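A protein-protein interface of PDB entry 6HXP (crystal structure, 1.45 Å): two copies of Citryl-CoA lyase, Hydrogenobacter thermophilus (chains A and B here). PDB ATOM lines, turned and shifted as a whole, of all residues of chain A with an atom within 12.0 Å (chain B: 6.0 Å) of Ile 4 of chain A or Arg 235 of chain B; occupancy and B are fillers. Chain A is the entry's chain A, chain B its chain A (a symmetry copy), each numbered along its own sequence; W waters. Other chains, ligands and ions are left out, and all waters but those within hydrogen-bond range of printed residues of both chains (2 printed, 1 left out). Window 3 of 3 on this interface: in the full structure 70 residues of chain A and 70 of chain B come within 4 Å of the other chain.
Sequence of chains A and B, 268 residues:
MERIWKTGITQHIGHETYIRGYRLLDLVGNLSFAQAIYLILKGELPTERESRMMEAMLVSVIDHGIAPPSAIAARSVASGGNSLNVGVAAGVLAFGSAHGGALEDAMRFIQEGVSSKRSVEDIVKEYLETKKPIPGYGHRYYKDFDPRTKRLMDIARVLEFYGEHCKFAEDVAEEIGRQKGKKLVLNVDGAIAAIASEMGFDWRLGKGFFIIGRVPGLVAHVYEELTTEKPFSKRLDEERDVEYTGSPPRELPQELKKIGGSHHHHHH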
ATOM      1  N   ARG A   3      -0.349 -20.125 -17.308  1.00  0.00           N
ATOM      2  CA  ARG A   3      -1.324 -19.035 -17.282  1.00  0.00           C
ATOM      3  C   ARG A   3      -0.837 -17.941 -16.333  1.00  0.00           C
ATOM      4  O   ARG A   3      -0.623 -18.200 -15.149  1.00  0.00           O
ATOM      5  CB  ARG A   3      -2.714 -19.559 -16.870  1.00  0.00           C
ATOM      6  CG  ARG A   3      -3.243 -20.597 -17.866  1.00  0.00           C
ATOM      7  CD  ARG A   3      -4.668 -21.033 -17.579  1.00  0.00           C
ATOM      8  NE  ARG A   3      -5.108 -22.081 -18.504  1.00  0.00           N
ATOM      9  CZ  ARG A   3      -6.368 -22.481 -18.648  1.00  0.00           C
ATOM     10  NH1 ARG A   3      -7.338 -21.913 -17.940  1.00  0.00           N
ATOM     11  NH2 ARG A   3      -6.670 -23.447 -19.508  1.00  0.00           N
ATOM     12  N   ILE A   4      -0.638 -16.731 -16.857  1.00  0.00           N
ATOM     13  CA  ILE A   4      -0.123 -15.610 -16.063  1.00  0.00           C
ATOM     14  C   ILE A   4      -1.231 -14.942 -15.258  1.00  0.00           C
ATOM     15  O   ILE A   4      -0.923 -14.254 -14.292  1.00  0.00           O
ATOM     16  CB  ILE A   4       0.702 -14.580 -16.904  1.00  0.00           C
ATOM     17  CG1 ILE A   4      -0.171 -13.568 -17.697  1.00  0.00           C
ATOM     18  CG2 ILE A   4       1.685 -15.313 -17.837  1.00  0.00           C
ATOM     19  CD1 ILE A   4       0.657 -12.440 -18.427  1.00  0.00           C
ATOM     20  N   TRP A   5      -2.498 -15.128 -15.650  1.00  0.00           N
ATOM     21  CA  TRP A   5      -3.631 -14.504 -14.978  1.00  0.00           C
ATOM     22  C   TRP A   5      -4.209 -15.507 -14.020  1.00  0.00           C
ATOM     23  O   TRP A   5      -4.950 -16.389 -14.431  1.00  0.00           O
ATOM     24  CB  TRP A   5      -4.641 -13.990 -16.017  1.00  0.00           C
ATOM     25  CG  TRP A   5      -4.052 -12.994 -16.966  1.00  0.00           C
ATOM     26  CD1 TRP A   5      -3.509 -13.248 -18.189  1.00  0.00           C
ATOM     27  CD2 TRP A   5      -3.880 -11.587 -16.733  1.00  0.00           C
ATOM     28  NE1 TRP A   5      -3.020 -12.079 -18.743  1.00  0.00           N
ATOM     29  CE2 TRP A   5      -3.279 -11.039 -17.885  1.00  0.00           C
ATOM     30  CE3 TRP A   5      -4.256 -10.727 -15.698  1.00  0.00           C
ATOM     31  CZ2 TRP A   5      -2.955  -9.679 -17.979  1.00  0.00           C
ATOM     32  CZ3 TRP A   5      -3.918  -9.387 -15.785  1.00  0.00           C
ATOM     33  CH2 TRP A   5      -3.371  -8.864 -16.945  1.00  0.00           C
ATOM     34  N   LYS A   6      -3.743 -15.465 -12.776  1.00  0.00           N
ATOM     35  CA  LYS A   6      -4.166 -16.384 -11.725  1.00  0.00           C
ATOM     36  C   LYS A   6      -4.922 -15.614 -10.688  1.00  0.00           C
ATOM     37  O   LYS A   6      -4.607 -14.451 -10.386  1.00  0.00           O
ATOM     38  CB  LYS A   6      -2.954 -17.030 -11.050  1.00  0.00           C
ATOM     39  CG  LYS A   6      -1.987 -17.692 -12.000  1.00  0.00           C
ATOM     40  CD  LYS A   6      -1.085 -18.675 -11.256  1.00  0.00           C
ATOM     41  CE  LYS A   6      -0.160 -18.043 -10.233  1.00  0.00           C
ATOM     42  NZ  LYS A   6       0.840 -17.119 -10.851  1.00  0.00           N
ATOM     43  N   THR A   7      -5.922 -16.270 -10.087  1.00  0.00           N
ATOM     44  CA  THR A   7      -6.685 -15.623  -9.051  1.00  0.00           C
ATOM     45  C   THR A   7      -7.443 -16.630  -8.206  1.00  0.00           C
ATOM     46  O   THR A   7      -7.839 -17.684  -8.720  1.00  0.00           O
ATOM     47  CB  THR A   7      -7.709 -14.619  -9.652  1.00  0.00           C
ATOM     48  OG1 THR A   7      -8.392 -13.940  -8.618  1.00  0.00           O
ATOM     49  CG2 THR A   7      -8.736 -15.291 -10.561  1.00  0.00           C
ATOM     50  N   GLY A   8      -7.631 -16.321  -6.939  1.00  0.00           N
ATOM     51  CA  GLY A   8      -8.446 -17.109  -6.029  1.00  0.00           C
ATOM     52  C   GLY A   8      -9.660 -16.336  -5.570  1.00  0.00           C
ATOM     53  O   GLY A   8     -10.329 -16.730  -4.612  1.00  0.00           O
ATOM     54  N   ILE A   9     -10.001 -15.198  -6.246  1.00  0.00           N
ATOM     55  CA  ILE A   9     -11.083 -14.368  -5.801  1.00  0.00           C
ATOM     56  C   ILE A   9     -12.420 -14.782  -6.329  1.00  0.00           C
ATOM     57  O   ILE A   9     -13.373 -14.984  -5.548  1.00  0.00           O
ATOM     58  CB  ILE A   9     -10.808 -12.878  -6.161  1.00  0.00           C
ATOM     59  CG1 ILE A   9      -9.490 -12.387  -5.597  1.00  0.00           C
ATOM     60  CG2 ILE A   9     -11.971 -11.969  -5.649  1.00  0.00           C
ATOM     61  CD1 ILE A   9      -9.011 -11.098  -6.236  1.00  0.00           C
ATOM     62  N   SER B  79       1.243  -4.314 -11.097  1.00  0.00           N
ATOM     63  CA  SER B  79       2.436  -5.042 -11.568  1.00  0.00           C
ATOM     64  C   SER B  79       3.624  -4.096 -11.876  1.00  0.00           C
ATOM     65  O   SER B  79       4.808  -4.490 -11.778  1.00  0.00           O
ATOM     66  CB  SER B  79       2.081  -5.880 -12.786  1.00  0.00           C
ATOM     67  OG  SER B  79       3.093  -6.867 -13.042  1.00  0.00           O
ATOM     68  N   GLU B 225      -2.687  -9.185  -6.641  1.00  0.00           N
ATOM     69  CA  GLU B 225      -1.567  -9.019  -7.556  1.00  0.00           C
ATOM     70  C   GLU B 225      -0.287  -8.603  -6.771  1.00  0.00           C
ATOM     71  O   GLU B 225       0.801  -9.112  -7.041  1.00  0.00           O
ATOM     72  CB  GLU B 225      -1.881  -7.943  -8.595  1.00  0.00           C
ATOM     73  CG  GLU B 225      -0.854  -7.856  -9.715  1.00  0.00           C
ATOM     74  CD  GLU B 225      -0.827  -9.051 -10.650  1.00  0.00           C
ATOM     75  OE1 GLU B 225      -1.903  -9.664 -10.868  1.00  0.00           O
ATOM     76  OE2 GLU B 225       0.264  -9.367 -11.193  1.00  0.00           O
ATOM     77  N   GLU B 229       2.160 -12.158  -6.752  1.00  0.00           N
ATOM     78  CA  GLU B 229       2.832 -12.184  -8.026  1.00  0.00           C
ATOM     79  C   GLU B 229       4.080 -11.357  -7.949  1.00  0.00           C
ATOM     80  O   GLU B 229       4.161 -10.392  -7.176  1.00  0.00           O
ATOM     81  CB  GLU B 229       1.910 -11.602  -9.111  1.00  0.00           C
ATOM     82  CG  GLU B 229       0.597 -12.362  -9.293  1.00  0.00           C
ATOM     83  CD  GLU B 229       0.742 -13.711  -9.973  1.00  0.00           C
ATOM     84  OE1 GLU B 229       1.858 -14.037 -10.434  1.00  0.00           O
ATOM     85  OE2 GLU B 229      -0.285 -14.413 -10.101  1.00  0.00           O
ATOM     86  N   PRO B 231       6.651  -8.560  -9.122  1.00  0.00           N
ATOM     87  CA  PRO B 231       6.495  -7.334  -9.902  1.00  0.00           C
ATOM     88  C   PRO B 231       6.896  -7.556 -11.357  1.00  0.00           C
ATOM     89  O   PRO B 231       7.804  -8.345 -11.693  1.00  0.00           O
ATOM     90  CB  PRO B 231       7.438  -6.336  -9.216  1.00  0.00           C
ATOM     91  CG  PRO B 231       7.571  -6.875  -7.798  1.00  0.00           C
ATOM     92  CD  PRO B 231       7.561  -8.367  -7.970  1.00  0.00           C
ATOM     93  N   PHE B 232       6.177  -6.863 -12.232  1.00  0.00           N
ATOM     94  CA  PHE B 232       6.376  -6.881 -13.668  1.00  0.00           C
ATOM     95  C   PHE B 232       5.956  -8.196 -14.314  1.00  0.00           C
ATOM     96  O   PHE B 232       6.236  -8.401 -15.493  1.00  0.00           O
ATOM     97  CB  PHE B 232       7.829  -6.502 -14.046  1.00  0.00           C
ATOM     98  CG  PHE B 232       7.945  -5.663 -15.307  1.00  0.00           C
ATOM     99  CD1 PHE B 232       7.428  -4.381 -15.360  1.00  0.00           C
ATOM    100  CD2 PHE B 232       8.576  -6.162 -16.435  1.00  0.00           C
ATOM    101  CE1 PHE B 232       7.566  -3.604 -16.512  1.00  0.00           C
ATOM    102  CE2 PHE B 232       8.752  -5.360 -17.575  1.00  0.00           C
ATOM    103  CZ  PHE B 232       8.205  -4.103 -17.618  1.00  0.00           C
ATOM    104  N   SER B 233       5.197  -9.062 -13.597  1.00  0.00           N
ATOM    105  CA  SER B 233       4.749 -10.309 -14.184  1.00  0.00           C
ATOM    106  C   SER B 233       3.664 -10.104 -15.241  1.00  0.00           C
ATOM    107  O   SER B 233       3.504 -10.978 -16.099  1.00  0.00           O
ATOM    108  CB  SER B 233       4.289 -11.282 -13.102  1.00  0.00           C
ATOM    109  OG  SER B 233       3.114 -10.842 -12.478  1.00  0.00           O
ATOM    110  N   LYS B 234       2.936  -8.976 -15.208  1.00  0.00           N
ATOM    111  CA  LYS B 234       1.870  -8.720 -16.192  1.00  0.00           C
ATOM    112  C   LYS B 234       2.433  -7.993 -17.404  1.00  0.00           C
ATOM    113  O   LYS B 234       2.458  -6.758 -17.496  1.00  0.00           O
ATOM    114  CB  LYS B 234       0.712  -7.931 -15.585  1.00  0.00           C
ATOM    115  CG  LYS B 234       0.024  -8.713 -14.476  1.00  0.00           C
ATOM    116  CD  LYS B 234      -0.534 -10.081 -14.946  1.00  0.00           C
ATOM    117  CE  LYS B 234      -1.378 -10.832 -13.928  1.00  0.00           C
ATOM    118  NZ  LYS B 234      -0.530 -11.460 -12.890  1.00  0.00           N
ATOM    119  N   ARG B 235       2.957  -8.791 -18.301  1.00  0.00           N
ATOM    120  CA  ARG B 235       3.555  -8.313 -19.539  1.00  0.00           C
ATOM    121  C   ARG B 235       3.291  -9.367 -20.580  1.00  0.00           C
ATOM    122  O   ARG B 235       3.164 -10.560 -20.242  1.00  0.00           O
ATOM    123  CB  ARG B 235       5.054  -8.057 -19.376  1.00  0.00           C
ATOM    124  CG  ARG B 235       5.888  -9.292 -19.059  1.00  0.00           C
ATOM    125  CD  ARG B 235       7.364  -8.922 -19.009  1.00  0.00           C
ATOM    126  NE  ARG B 235       8.199 -10.116 -18.850  1.00  0.00           N
ATOM    127  CZ  ARG B 235       8.545 -10.651 -17.681  1.00  0.00           C
ATOM    128  NH1 ARG B 235       9.293 -11.747 -17.641  1.00  0.00           N
ATOM    129  NH2 ARG B 235       8.153 -10.091 -16.544  1.00  0.00           N
ATOM    130  N   LEU B 236       3.099  -8.959 -21.809  1.00  0.00           N
ATOM    131  CA  LEU B 236       2.849  -9.917 -22.885  1.00  0.00           C
ATOM    132  C   LEU B 236       4.167 -10.487 -23.383  1.00  0.00           C
ATOM    133  O   LEU B 236       5.231  -9.959 -23.092  1.00  0.00           O
ATOM    134  CB  LEU B 236       2.136  -9.254 -24.070  1.00  0.00           C
ATOM    135  CG  LEU B 236       0.881  -8.433 -23.774  1.00  0.00           C
ATOM    136  CD1 LEU B 236       0.333  -7.860 -25.066  1.00  0.00           C
ATOM    137  CD2 LEU B 236      -0.174  -9.247 -23.039  1.00  0.00           C
ATOM    138  N   ASP B 237       4.069 -11.596 -24.131  1.00  0.00           N
ATOM    139  CA  ASP B 237       5.197 -12.234 -24.836  1.00  0.00           C
ATOM    140  C   ASP B 237       4.909 -11.894 -26.302  1.00  0.00           C
ATOM    141  O   ASP B 237       3.893 -12.335 -26.840  1.00  0.00           O
ATOM    142  CB  ASP B 237       5.169 -13.736 -24.575  1.00  0.00           C
ATOM    143  CG  ASP B 237       6.134 -14.579 -25.392  1.00  0.00           C
ATOM    144  OD1 ASP B 237       7.041 -14.000 -26.038  1.00  0.00           O
ATOM    145  OD2 ASP B 237       6.002 -15.810 -25.362  1.00  0.00           O
ATOM    146  N   ARG B 240       4.563 -14.733 -28.937  1.00  0.00           N
ATOM    147  CA  ARG B 240       3.400 -15.587 -28.707  1.00  0.00           C
ATOM    148  C   ARG B 240       2.029 -14.909 -28.720  1.00  0.00           C
ATOM    149  O   ARG B 240       1.054 -15.501 -29.164  1.00  0.00           O
ATOM    150  CB  ARG B 240       3.591 -16.270 -27.340  1.00  0.00           C
ATOM    151  CG  ARG B 240       2.514 -17.269 -26.926  1.00  0.00           C
ATOM    152  CD  ARG B 240       2.922 -18.039 -25.676  1.00  0.00           C
ATOM    153  NE  ARG B 240       3.273 -17.153 -24.561  1.00  0.00           N
ATOM    154  CZ  ARG B 240       2.392 -16.564 -23.759  1.00  0.00           C
ATOM    155  NH1 ARG B 240       1.091 -16.762 -23.930  1.00  0.00           N
ATOM    156  NH2 ARG B 240       2.805 -15.769 -22.781  1.00  0.00           N
ATOM    157  N   ASP B 241       1.930 -13.700 -28.147  1.00  0.00           N
ATOM    158  CA  ASP B 241       0.651 -13.015 -27.913  1.00  0.00           C
ATOM    159  C   ASP B 241       0.279 -11.898 -28.841  1.00  0.00           C
ATOM    160  O   ASP B 241      -0.863 -11.435 -28.775  1.00  0.00           O
ATOM    161  CB  ASP B 241       0.679 -12.389 -26.509  1.00  0.00           C
ATOM    162  CG  ASP B 241       0.968 -13.407 -25.424  1.00  0.00           C
ATOM    163  OD1 ASP B 241       0.577 -14.594 -25.603  1.00  0.00           O
ATOM    164  OD2 ASP B 241       1.630 -13.037 -24.423  1.00  0.00           O
HETATM  165  O   HOH W   1      -2.903 -13.921  -8.377  1.00  0.00           O
HETATM  166  O   HOH W   2       1.593 -13.278 -13.485  1.00  0.00           O
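Ile 4 of chain A touches Ser 233 of chain B.
CD1 of Ile 4 of chain A touches O of Arg 235 of chain B, 3.6 Å away.
Trp 5 of chain A touches Lys 234 of chain B.
O of Phe 232 of chain B is in hydrogen-bond range of NH2 of Arg 235 of chain B.
The side-chain carboxylate (OE2) of Glu 225 of chain B is in salt-bridge range of the side-chain amino group (NZ) of Lys 234 of chain B, 2.8 Å away.
The backbone NH (N) of Ser 233 of chain B lies within hydrogen-bond range of the side-chain hydroxyl (OG) of Ser 79 of chain B (3.1 Å).
The side-chain hydroxyl (OG) of Ser 79 of chain B lies within hydrogen-bond range of the backbone NH (N) of Lys 234 of chain B (3.0 Å).
OE2 of Glu 225 of chain B is in hydrogen-bond range of OG of Ser 233 of chain B.
The side-chain amino group (NZ) of Lys 6 of chain A is in salt-bridge range of the side-chain carboxylate (OE2) of Glu 229 of chain B.
The backbone carbonyl oxygen of Ile 4 of chain A sits at hydrogen-bond distance from the side-chain amino group of Lys 234 of chain B (3.2 Å).
Of chain B, only Ser 233, Lys 234 and Arg 235 come within 4 Å of Ile 4 of chain A.
Of the printed residues of chain B, Trp 5 of chain A touches Lys 234 (3.4 Å).
Printed residues of chain B within 4 Å of Lys 6 of chain A: Glu 229 (3.0 Å).
Ile 9 of chain A touches none of the printed residues of chain B.
Of the printed residues of chain A, Glu 229 of chain B touches Lys 6 (3.0 Å).
No residue of chain A comes within 4 Å of Phe 232 of chain B.
Lys 234 of chain B touches just these residues of chain A: Ile 4 (3.2 Å) and Trp 5 (3.4 Å).
Of the printed residues of chain A, Arg 235 of chain B touches Ile 4 (3.6 Å).
Leu 236 of chain B touches none of the printed residues of chain A.
No residue of chain A comes within 4 Å of Asp 237 of chain B.
The nearest residue of chain B that does not touch Ile 4 of chain A is Glu 229 of chain B (4.2 Å).
The nearest residue of chain A that does not touch Arg 235 of chain B is Trp 5 of chain A (6.0 Å).
The nearest printed residue of chain B that does not touch Trp 5 of chain A is Glu 225 of chain B (5.3 Å).
Printed residues of chain B that touch a printed residue of chain A: Glu 229, Ser 233, Lys 234 and Arg 235.
Among the printed residues, 5 pairs touch across the chains.
Among the printed residues, Asp or Glu carboxylates within 4 Å of a Lys or Arg side-chain nitrogen of the other chain: Lys 6 of chain A with Glu 229 of chain B (3.0 Å).
No position is printed for both chains.
Of the 5 pairs that touch across the chains among the printed residues, none has its exchanged pair printed and touching as well.
Water W1 bridges the backbone carbonyl oxygen (O) of Lys 6 of chain A (2.7 Å) and the side-chain carboxylate (OE2) of Glu 229 of chain B (3.2 Å).
Water W2 lies within hydrogen-bond range of O of Ile 4 of chain A, NZ of Lys 234 of chain B, OG of Ser 233 of chain B and OE1 of Glu 229 of chain B.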
